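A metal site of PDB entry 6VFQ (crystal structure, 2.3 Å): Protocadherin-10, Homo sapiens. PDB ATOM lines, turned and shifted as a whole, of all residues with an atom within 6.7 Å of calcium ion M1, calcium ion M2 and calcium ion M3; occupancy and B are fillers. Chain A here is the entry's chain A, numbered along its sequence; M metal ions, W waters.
OD2 of Asp 97 is in hydrogen-bond range of ND2 of Asn 137 (2.9 Å). OD1 of Asp 100 lies close to ND2 of Asn 101 (3.3 Å). The side-chain amide nitrogen (ND2) of Asn 101 sits close to the side-chain carboxylate (OE2) of Glu 65. The side-chain carboxylate of Glu 65 sits close to the guanidinium group of Arg 64, 2.6 Å away. OE1 of Glu 9 sits close to N of Arg 64. The side-chain hydroxyl (OG) of Ser 138 sits at hydrogen-bond distance from the backbone carbonyl oxygen (O) of Asp 133. The side-chain carboxylate (OD1) of Asp 188 is in hydrogen-bond range of the backbone NH (N) of Arg 213, at 2.9 Å. N of Glu 10 sits at hydrogen-bond distance from O of Ile 62, at 2.6 Å.
The nearest printed residue that does not touch calcium ion M2 is Asn 99 (4.6 Å).
Calcium ion M3 is bound by O of Asn 101, O of Asn 137, OD2 of Asp 131, OD1 of Asn 99, OD2 of Asp 133, OD2 of Asp 188 and OD1 of Asp 131.
Calcium ion M1 is bound by the side-chain carboxylate (OD2) of Asp 100, 2.2 Å away. Calcium ion M1 is bound by OD1 of Asp 63 (2.3 Å). Calcium ion M1 is bound by the side-chain carboxylate (OE2) of Glu 65 (2.3 Å). Water W1 is bound to calcium ion M1, at 2.4 Å. OE1 of Glu 9 is bound to calcium ion M1 (2.4 Å). Calcium ion M1 is bound by the side-chain carboxylate (OE1) of Glu 10, at 2.5 Å. Calcium ion M1 has six donor atoms within binding distance.
Calcium ion M2 is bound by OD1 of Asp 97 (2.2 Å), OD1 of Asp 100 (2.2 Å), O of Ile 98 (2.4 Å), OE2 of Glu 9 (2.4 Å), OD1 of Asp 133 (2.4 Å), OE1 of Glu 65 (2.5 Å) and OE2 of Glu 65 (2.6 Å). Calcium ion M2 has seven donor atoms within binding distance.
Of the 27 residues printed, 5 come within 4 Å of calcium ion M1.
Of the 27 residues printed, 6 come within 4 Å of calcium ion M3.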
ATOM      1  N   GLU A   9       7.995  17.558 -20.099  1.00  0.00           N
ATOM      2  CA  GLU A   9       8.952  18.587 -19.718  1.00  0.00           C
ATOM      3  C   GLU A   9       8.925  19.689 -20.762  1.00  0.00           C
ATOM      4  O   GLU A   9       8.537  19.476 -21.907  1.00  0.00           O
ATOM      5  CB  GLU A   9      10.369  18.013 -19.601  1.00  0.00           C
ATOM      6  CG  GLU A   9      10.940  17.562 -20.938  1.00  0.00           C
ATOM      7  CD  GLU A   9      12.461  17.389 -20.920  1.00  0.00           C
ATOM      8  OE1 GLU A   9      13.181  18.241 -20.356  1.00  0.00           O
ATOM      9  OE2 GLU A   9      12.927  16.380 -21.487  1.00  0.00           O
ATOM     10  N   GLU A  10       9.303  20.884 -20.330  1.00  0.00           N
ATOM     11  CA  GLU A  10       9.438  22.044 -21.196  1.00  0.00           C
ATOM     12  C   GLU A  10       8.091  22.595 -21.689  1.00  0.00           C
ATOM     13  O   GLU A  10       8.042  23.267 -22.719  1.00  0.00           O
ATOM     14  CB  GLU A  10      10.345  21.724 -22.391  1.00  0.00           C
ATOM     15  CG  GLU A  10      11.683  21.059 -22.003  1.00  0.00           C
ATOM     16  CD  GLU A  10      12.642  21.946 -21.209  1.00  0.00           C
ATOM     17  OE1 GLU A  10      13.666  21.412 -20.705  1.00  0.00           O
ATOM     18  OE2 GLU A  10      12.405  23.178 -21.103  1.00  0.00           O
ATOM     19  N   ILE A  62       9.517  23.111 -16.760  1.00  0.00           N
ATOM     20  CA  ILE A  62      10.243  21.992 -16.176  1.00  0.00           C
ATOM     21  C   ILE A  62      11.280  21.490 -17.161  1.00  0.00           C
ATOM     22  O   ILE A  62      10.937  21.090 -18.282  1.00  0.00           O
ATOM     23  CB  ILE A  62       9.275  20.861 -15.779  1.00  0.00           C
ATOM     24  CG1 ILE A  62       8.204  21.389 -14.824  1.00  0.00           C
ATOM     25  CG2 ILE A  62      10.063  19.717 -15.160  1.00  0.00           C
ATOM     26  CD1 ILE A  62       7.104  20.377 -14.516  1.00  0.00           C
ATOM     27  N   ASP A  63      12.551  21.529 -16.768  1.00  0.00           N
ATOM     28  CA  ASP A  63      13.632  20.849 -17.490  1.00  0.00           C
ATOM     29  C   ASP A  63      13.923  19.551 -16.759  1.00  0.00           C
ATOM     30  O   ASP A  63      14.474  19.556 -15.649  1.00  0.00           O
ATOM     31  CB  ASP A  63      14.884  21.704 -17.581  1.00  0.00           C
ATOM     32  CG  ASP A  63      16.055  20.969 -18.261  1.00  0.00           C
ATOM     33  OD1 ASP A  63      15.830  19.923 -18.931  1.00  0.00           O
ATOM     34  OD2 ASP A  63      17.209  21.438 -18.119  1.00  0.00           O
ATOM     35  N   ARG A  64      13.498  18.441 -17.345  1.00  0.00           N
ATOM     36  CA  ARG A  64      13.705  17.152 -16.706  1.00  0.00           C
ATOM     37  C   ARG A  64      15.184  16.897 -16.468  1.00  0.00           C
ATOM     38  O   ARG A  64      15.567  16.349 -15.427  1.00  0.00           O
ATOM     39  CB  ARG A  64      13.108  16.037 -17.572  1.00  0.00           C
ATOM     40  CG  ARG A  64      12.920  14.706 -16.839  1.00  0.00           C
ATOM     41  CD  ARG A  64      12.972  13.555 -17.821  1.00  0.00           C
ATOM     42  NE  ARG A  64      14.288  13.627 -18.457  1.00  0.00           N
ATOM     43  CZ  ARG A  64      15.417  13.182 -17.916  1.00  0.00           C
ATOM     44  NH1 ARG A  64      15.407  12.563 -16.743  1.00  0.00           N
ATOM     45  NH2 ARG A  64      16.559  13.359 -18.563  1.00  0.00           N
ATOM     46  N   GLU A  65      16.045  17.285 -17.423  1.00  0.00           N
ATOM     47  CA  GLU A  65      17.465  17.007 -17.255  1.00  0.00           C
ATOM     48  C   GLU A  65      18.005  17.677 -16.014  1.00  0.00           C
ATOM     49  O   GLU A  65      18.976  17.202 -15.408  1.00  0.00           O
ATOM     50  CB  GLU A  65      18.266  17.443 -18.486  1.00  0.00           C
ATOM     51  CG  GLU A  65      18.136  16.501 -19.683  1.00  0.00           C
ATOM     52  CD  GLU A  65      16.728  16.417 -20.306  1.00  0.00           C
ATOM     53  OE1 GLU A  65      16.155  15.306 -20.272  1.00  0.00           O
ATOM     54  OE2 GLU A  65      16.214  17.437 -20.850  1.00  0.00           O
ATOM     55  N   GLN A  66      17.378  18.768 -15.583  1.00  0.00           N
ATOM     56  CA  GLN A  66      17.866  19.487 -14.415  1.00  0.00           C
ATOM     57  C   GLN A  66      17.360  18.871 -13.122  1.00  0.00           C
ATOM     58  O   GLN A  66      18.148  18.581 -12.213  1.00  0.00           O
ATOM     59  CB  GLN A  66      17.483  20.954 -14.499  1.00  0.00           C
ATOM     60  CG  GLN A  66      17.817  21.697 -13.222  1.00  0.00           C
ATOM     61  CD  GLN A  66      17.966  23.169 -13.463  1.00  0.00           C
ATOM     62  OE1 GLN A  66      18.344  23.591 -14.544  1.00  0.00           O
ATOM     63  NE2 GLN A  66      17.647  23.967 -12.449  1.00  0.00           N
ATOM     64  N   LEU A  96       7.636  13.594 -18.198  1.00  0.00           N
ATOM     65  CA  LEU A  96       8.087  12.785 -19.302  1.00  0.00           C
ATOM     66  C   LEU A  96       9.214  13.483 -20.056  1.00  0.00           C
ATOM     67  O   LEU A  96       9.135  14.687 -20.327  1.00  0.00           O
ATOM     68  CB  LEU A  96       6.936  12.523 -20.265  1.00  0.00           C
ATOM     69  CG  LEU A  96       5.678  11.973 -19.589  1.00  0.00           C
ATOM     70  CD1 LEU A  96       4.551  11.849 -20.594  1.00  0.00           C
ATOM     71  CD2 LEU A  96       5.979  10.641 -18.920  1.00  0.00           C
ATOM     72  N   ASP A  97      10.258  12.719 -20.391  1.00  0.00           N
ATOM     73  CA  ASP A  97      11.415  13.235 -21.123  1.00  0.00           C
ATOM     74  C   ASP A  97      11.078  13.439 -22.597  1.00  0.00           C
ATOM     75  O   ASP A  97      10.464  12.569 -23.221  1.00  0.00           O
ATOM     76  CB  ASP A  97      12.592  12.263 -20.999  1.00  0.00           C
ATOM     77  CG  ASP A  97      13.806  12.650 -21.864  1.00  0.00           C
ATOM     78  OD1 ASP A  97      14.301  13.814 -21.780  1.00  0.00           O
ATOM     79  OD2 ASP A  97      14.283  11.757 -22.615  1.00  0.00           O
ATOM     80  N   ILE A  98      11.478  14.579 -23.145  1.00  0.00           N
ATOM     81  CA  ILE A  98      11.511  14.737 -24.598  1.00  0.00           C
ATOM     82  C   ILE A  98      12.968  14.740 -25.077  1.00  0.00           C
ATOM     83  O   ILE A  98      13.909  14.862 -24.288  1.00  0.00           O
ATOM     84  CB  ILE A  98      10.774  16.007 -25.060  1.00  0.00           C
ATOM     85  CG1 ILE A  98      11.396  17.242 -24.426  1.00  0.00           C
ATOM     86  CG2 ILE A  98       9.318  15.934 -24.714  1.00  0.00           C
ATOM     87  CD1 ILE A  98      10.796  18.555 -24.934  1.00  0.00           C
ATOM     88  N   ASN A  99      13.134  14.624 -26.398  1.00  0.00           N
ATOM     89  CA  ASN A  99      14.452  14.556 -27.025  1.00  0.00           C
ATOM     90  C   ASN A  99      14.913  15.955 -27.410  1.00  0.00           C
ATOM     91  O   ASN A  99      14.986  16.314 -28.590  1.00  0.00           O
ATOM     92  CB  ASN A  99      14.430  13.662 -28.255  1.00  0.00           C
ATOM     93  CG  ASN A  99      15.837  13.271 -28.699  1.00  0.00           C
ATOM     94  OD1 ASN A  99      16.725  13.136 -27.868  1.00  0.00           O
ATOM     95  ND2 ASN A  99      16.044  13.076 -30.003  1.00  0.00           N
ATOM     96  N   ASP A 100      15.231  16.750 -26.387  1.00  0.00           N
ATOM     97  CA  ASP A 100      15.733  18.110 -26.569  1.00  0.00           C
ATOM     98  C   ASP A 100      17.250  18.218 -26.410  1.00  0.00           C
ATOM     99  O   ASP A 100      17.767  19.331 -26.258  1.00  0.00           O
ATOM    100  CB  ASP A 100      15.013  19.063 -25.601  1.00  0.00           C
ATOM    101  CG  ASP A 100      14.981  18.560 -24.169  1.00  0.00           C
ATOM    102  OD1 ASP A 100      15.113  17.334 -23.972  1.00  0.00           O
ATOM    103  OD2 ASP A 100      14.779  19.394 -23.241  1.00  0.00           O
ATOM    104  N   ASN A 101      18.000  17.104 -26.458  1.00  0.00           N
ATOM    105  CA  ASN A 101      19.457  17.187 -26.355  1.00  0.00           C
ATOM    106  C   ASN A 101      20.104  16.214 -27.330  1.00  0.00           C
ATOM    107  O   ASN A 101      19.665  15.036 -27.422  1.00  0.00           O
ATOM    108  CB  ASN A 101      19.984  16.900 -24.951  1.00  0.00           C
ATOM    109  CG  ASN A 101      19.482  17.900 -23.944  1.00  0.00           C
ATOM    110  OD1 ASN A 101      20.119  18.907 -23.687  1.00  0.00           O
ATOM    111  ND2 ASN A 101      18.321  17.630 -23.386  1.00  0.00           N
ATOM    112  N   PRO A 102      21.131  16.648 -28.050  1.00  0.00           N
ATOM    113  CA  PRO A 102      21.866  15.734 -28.909  1.00  0.00           C
ATOM    114  C   PRO A 102      22.893  14.980 -28.090  1.00  0.00           C
ATOM    115  O   PRO A 102      23.276  15.404 -26.988  1.00  0.00           O
ATOM    116  CB  PRO A 102      22.542  16.670 -29.914  1.00  0.00           C
ATOM    117  CG  PRO A 102      22.859  17.910 -29.065  1.00  0.00           C
ATOM    118  CD  PRO A 102      21.780  17.971 -27.978  1.00  0.00           C
ATOM    119  N   PRO A 103      23.390  13.853 -28.582  1.00  0.00           N
ATOM    120  CA  PRO A 103      24.632  13.321 -28.030  1.00  0.00           C
ATOM    121  C   PRO A 103      25.754  14.327 -28.278  1.00  0.00           C
ATOM    122  O   PRO A 103      25.734  15.087 -29.255  1.00  0.00           O
ATOM    123  CB  PRO A 103      24.833  12.011 -28.782  1.00  0.00           C
ATOM    124  CG  PRO A 103      23.926  12.087 -29.948  1.00  0.00           C
ATOM    125  CD  PRO A 103      22.812  12.986 -29.612  1.00  0.00           C
ATOM    126  N   ASP A 131      24.647  11.780 -23.894  1.00  0.00           N
ATOM    127  CA  ASP A 131      23.340  12.344 -24.242  1.00  0.00           C
ATOM    128  C   ASP A 131      22.528  12.472 -22.959  1.00  0.00           C
ATOM    129  O   ASP A 131      22.235  11.444 -22.329  1.00  0.00           O
ATOM    130  CB  ASP A 131      22.603  11.475 -25.245  1.00  0.00           C
ATOM    131  CG  ASP A 131      21.366  12.160 -25.832  1.00  0.00           C
ATOM    132  OD1 ASP A 131      20.600  12.771 -25.058  1.00  0.00           O
ATOM    133  OD2 ASP A 131      21.182  12.096 -27.069  1.00  0.00           O
ATOM    134  N   PRO A 132      22.178  13.673 -22.521  1.00  0.00           N
ATOM    135  CA  PRO A 132      21.548  13.803 -21.189  1.00  0.00           C
ATOM    136  C   PRO A 132      20.095  13.328 -21.124  1.00  0.00           C
ATOM    137  O   PRO A 132      19.598  13.114 -20.016  1.00  0.00           O
ATOM    138  CB  PRO A 132      21.648  15.305 -20.899  1.00  0.00           C
ATOM    139  CG  PRO A 132      21.683  15.941 -22.253  1.00  0.00           C
ATOM    140  CD  PRO A 132      22.391  14.970 -23.168  1.00  0.00           C
ATOM    141  N   ASP A 133      19.397  13.178 -22.248  1.00  0.00           N
ATOM    142  CA  ASP A 133      18.055  12.630 -22.242  1.00  0.00           C
ATOM    143  C   ASP A 133      18.113  11.184 -21.778  1.00  0.00           C
ATOM    144  O   ASP A 133      19.202  10.607 -21.653  1.00  0.00           O
ATOM    145  CB  ASP A 133      17.443  12.718 -23.637  1.00  0.00           C
ATOM    146  CG  ASP A 133      17.418  14.132 -24.151  1.00  0.00           C
ATOM    147  OD1 ASP A 133      17.146  15.054 -23.358  1.00  0.00           O
ATOM    148  OD2 ASP A 133      17.704  14.308 -25.354  1.00  0.00           O
ATOM    149  N   VAL A 134      16.950  10.580 -21.521  1.00  0.00           N
ATOM    150  CA  VAL A 134      16.900   9.222 -20.967  1.00  0.00           C
ATOM    151  C   VAL A 134      16.204   8.282 -21.938  1.00  0.00           C
ATOM    152  O   VAL A 134      15.579   8.687 -22.920  1.00  0.00           O
ATOM    153  CB  VAL A 134      16.215   9.169 -19.590  1.00  0.00           C
ATOM    154  CG1 VAL A 134      17.100   9.786 -18.535  1.00  0.00           C
ATOM    155  CG2 VAL A 134      14.828   9.875 -19.611  1.00  0.00           C
ATOM    156  N   THR A 136      15.075   5.835 -24.746  1.00  0.00           N
ATOM    157  CA  THR A 136      15.251   5.855 -26.190  1.00  0.00           C
ATOM    158  C   THR A 136      15.786   7.190 -26.682  1.00  0.00           C
ATOM    159  O   THR A 136      16.353   7.254 -27.771  1.00  0.00           O
ATOM    160  CB  THR A 136      13.927   5.530 -26.893  1.00  0.00           C
ATOM    161  OG1 THR A 136      14.176   5.253 -28.275  1.00  0.00           O
ATOM    162  CG2 THR A 136      12.956   6.689 -26.807  1.00  0.00           C
ATOM    163  N   ASN A 137      15.597   8.274 -25.925  1.00  0.00           N
ATOM    164  CA  ASN A 137      16.117   9.573 -26.316  1.00  0.00           C
ATOM    165  C   ASN A 137      17.608   9.725 -26.068  1.00  0.00           C
ATOM    166  O   ASN A 137      18.194  10.751 -26.459  1.00  0.00           O
ATOM    167  CB  ASN A 137      15.353  10.666 -25.573  1.00  0.00           C
ATOM    168  CG  ASN A 137      13.932  10.745 -26.029  1.00  0.00           C
ATOM    169  OD1 ASN A 137      13.634  10.500 -27.201  1.00  0.00           O
ATOM    170  ND2 ASN A 137      13.029  11.082 -25.106  1.00  0.00           N
ATOM    171  N   SER A 138      18.224   8.759 -25.406  1.00  0.00           N
ATOM    172  CA  SER A 138      19.650   8.807 -25.125  1.00  0.00           C
ATOM    173  C   SER A 138      20.457   8.200 -26.268  1.00  0.00           C
ATOM    174  O   SER A 138      19.927   7.784 -27.297  1.00  0.00           O
ATOM    175  CB  SER A 138      19.953   8.094 -23.817  1.00  0.00           C
ATOM    176  OG  SER A 138      21.156   8.607 -23.250  1.00  0.00           O
ATOM    177  N   LEU A 139      21.771   8.146 -26.062  1.00  0.00           N
ATOM    178  CA  LEU A 139      22.693   7.649 -27.064  1.00  0.00           C
ATOM    179  C   LEU A 139      22.315   6.248 -27.526  1.00  0.00           C
ATOM    180  O   LEU A 139      22.048   5.368 -26.711  1.00  0.00           O
ATOM    181  CB  LEU A 139      24.097   7.664 -26.466  1.00  0.00           C
ATOM    182  CG  LEU A 139      25.215   7.120 -27.343  1.00  0.00           C
ATOM    183  CD1 LEU A 139      25.467   8.070 -28.511  1.00  0.00           C
ATOM    184  CD2 LEU A 139      26.444   6.975 -26.470  1.00  0.00           C
ATOM    185  N   ASP A 188      21.273   9.504 -31.129  1.00  0.00           N
ATOM    186  CA  ASP A 188      20.406   8.976 -30.094  1.00  0.00           C
ATOM    187  C   ASP A 188      19.283   8.198 -30.774  1.00  0.00           C
ATOM    188  O   ASP A 188      19.331   7.934 -31.975  1.00  0.00           O
ATOM    189  CB  ASP A 188      19.906  10.096 -29.170  1.00  0.00           C
ATOM    190  CG  ASP A 188      19.086  11.174 -29.896  1.00  0.00           C
ATOM    191  OD1 ASP A 188      18.566  10.929 -31.008  1.00  0.00           O
ATOM    192  OD2 ASP A 188      18.936  12.271 -29.320  1.00  0.00           O
ATOM    193  N   GLY A 189      18.259   7.817 -30.009  1.00  0.00           N
ATOM    194  CA  GLY A 189      17.237   6.917 -30.525  1.00  0.00           C
ATOM    195  C   GLY A 189      15.880   7.555 -30.740  1.00  0.00           C
ATOM    196  O   GLY A 189      14.860   6.876 -30.581  1.00  0.00           O
ATOM    197  N   GLY A 190      15.839   8.829 -31.103  1.00  0.00           N
ATOM    198  CA  GLY A 190      14.580   9.495 -31.328  1.00  0.00           C
ATOM    199  C   GLY A 190      14.104   9.425 -32.768  1.00  0.00           C
ATOM    200  O   GLY A 190      14.468  10.279 -33.587  1.00  0.00           O
ATOM    201  N   ARG A 213      18.555  13.083 -32.952  1.00  0.00           N
ATOM    202  CA  ARG A 213      19.605  14.090 -32.871  1.00  0.00           C
ATOM    203  C   ARG A 213      20.974  13.431 -32.961  1.00  0.00           C
ATOM    204  O   ARG A 213      21.144  12.240 -32.674  1.00  0.00           O
ATOM    205  CB  ARG A 213      19.450  14.908 -31.591  1.00  0.00           C
ATOM    206  CG  ARG A 213      18.022  15.423 -31.437  1.00  0.00           C
ATOM    207  CD  ARG A 213      17.821  16.393 -30.272  1.00  0.00           C
ATOM    208  NE  ARG A 213      18.034  17.766 -30.706  1.00  0.00           N
ATOM    209  CZ  ARG A 213      17.083  18.619 -31.045  1.00  0.00           C
ATOM    210  NH1 ARG A 213      15.808  18.263 -30.986  1.00  0.00           N
ATOM    211  NH2 ARG A 213      17.403  19.847 -31.433  1.00  0.00           N
HETATM  212 CA    CA M   1      15.166  19.441 -21.037  1.00  0.00          CA
HETATM  213 CA    CA M   2      15.032  15.765 -22.420  1.00  0.00          CA
HETATM  214 CA    CA M   3      18.939  12.923 -26.942  1.00  0.00          CA
HETATM  215  O   HOH W   1      17.226  20.256 -21.980  1.00  0.00           O
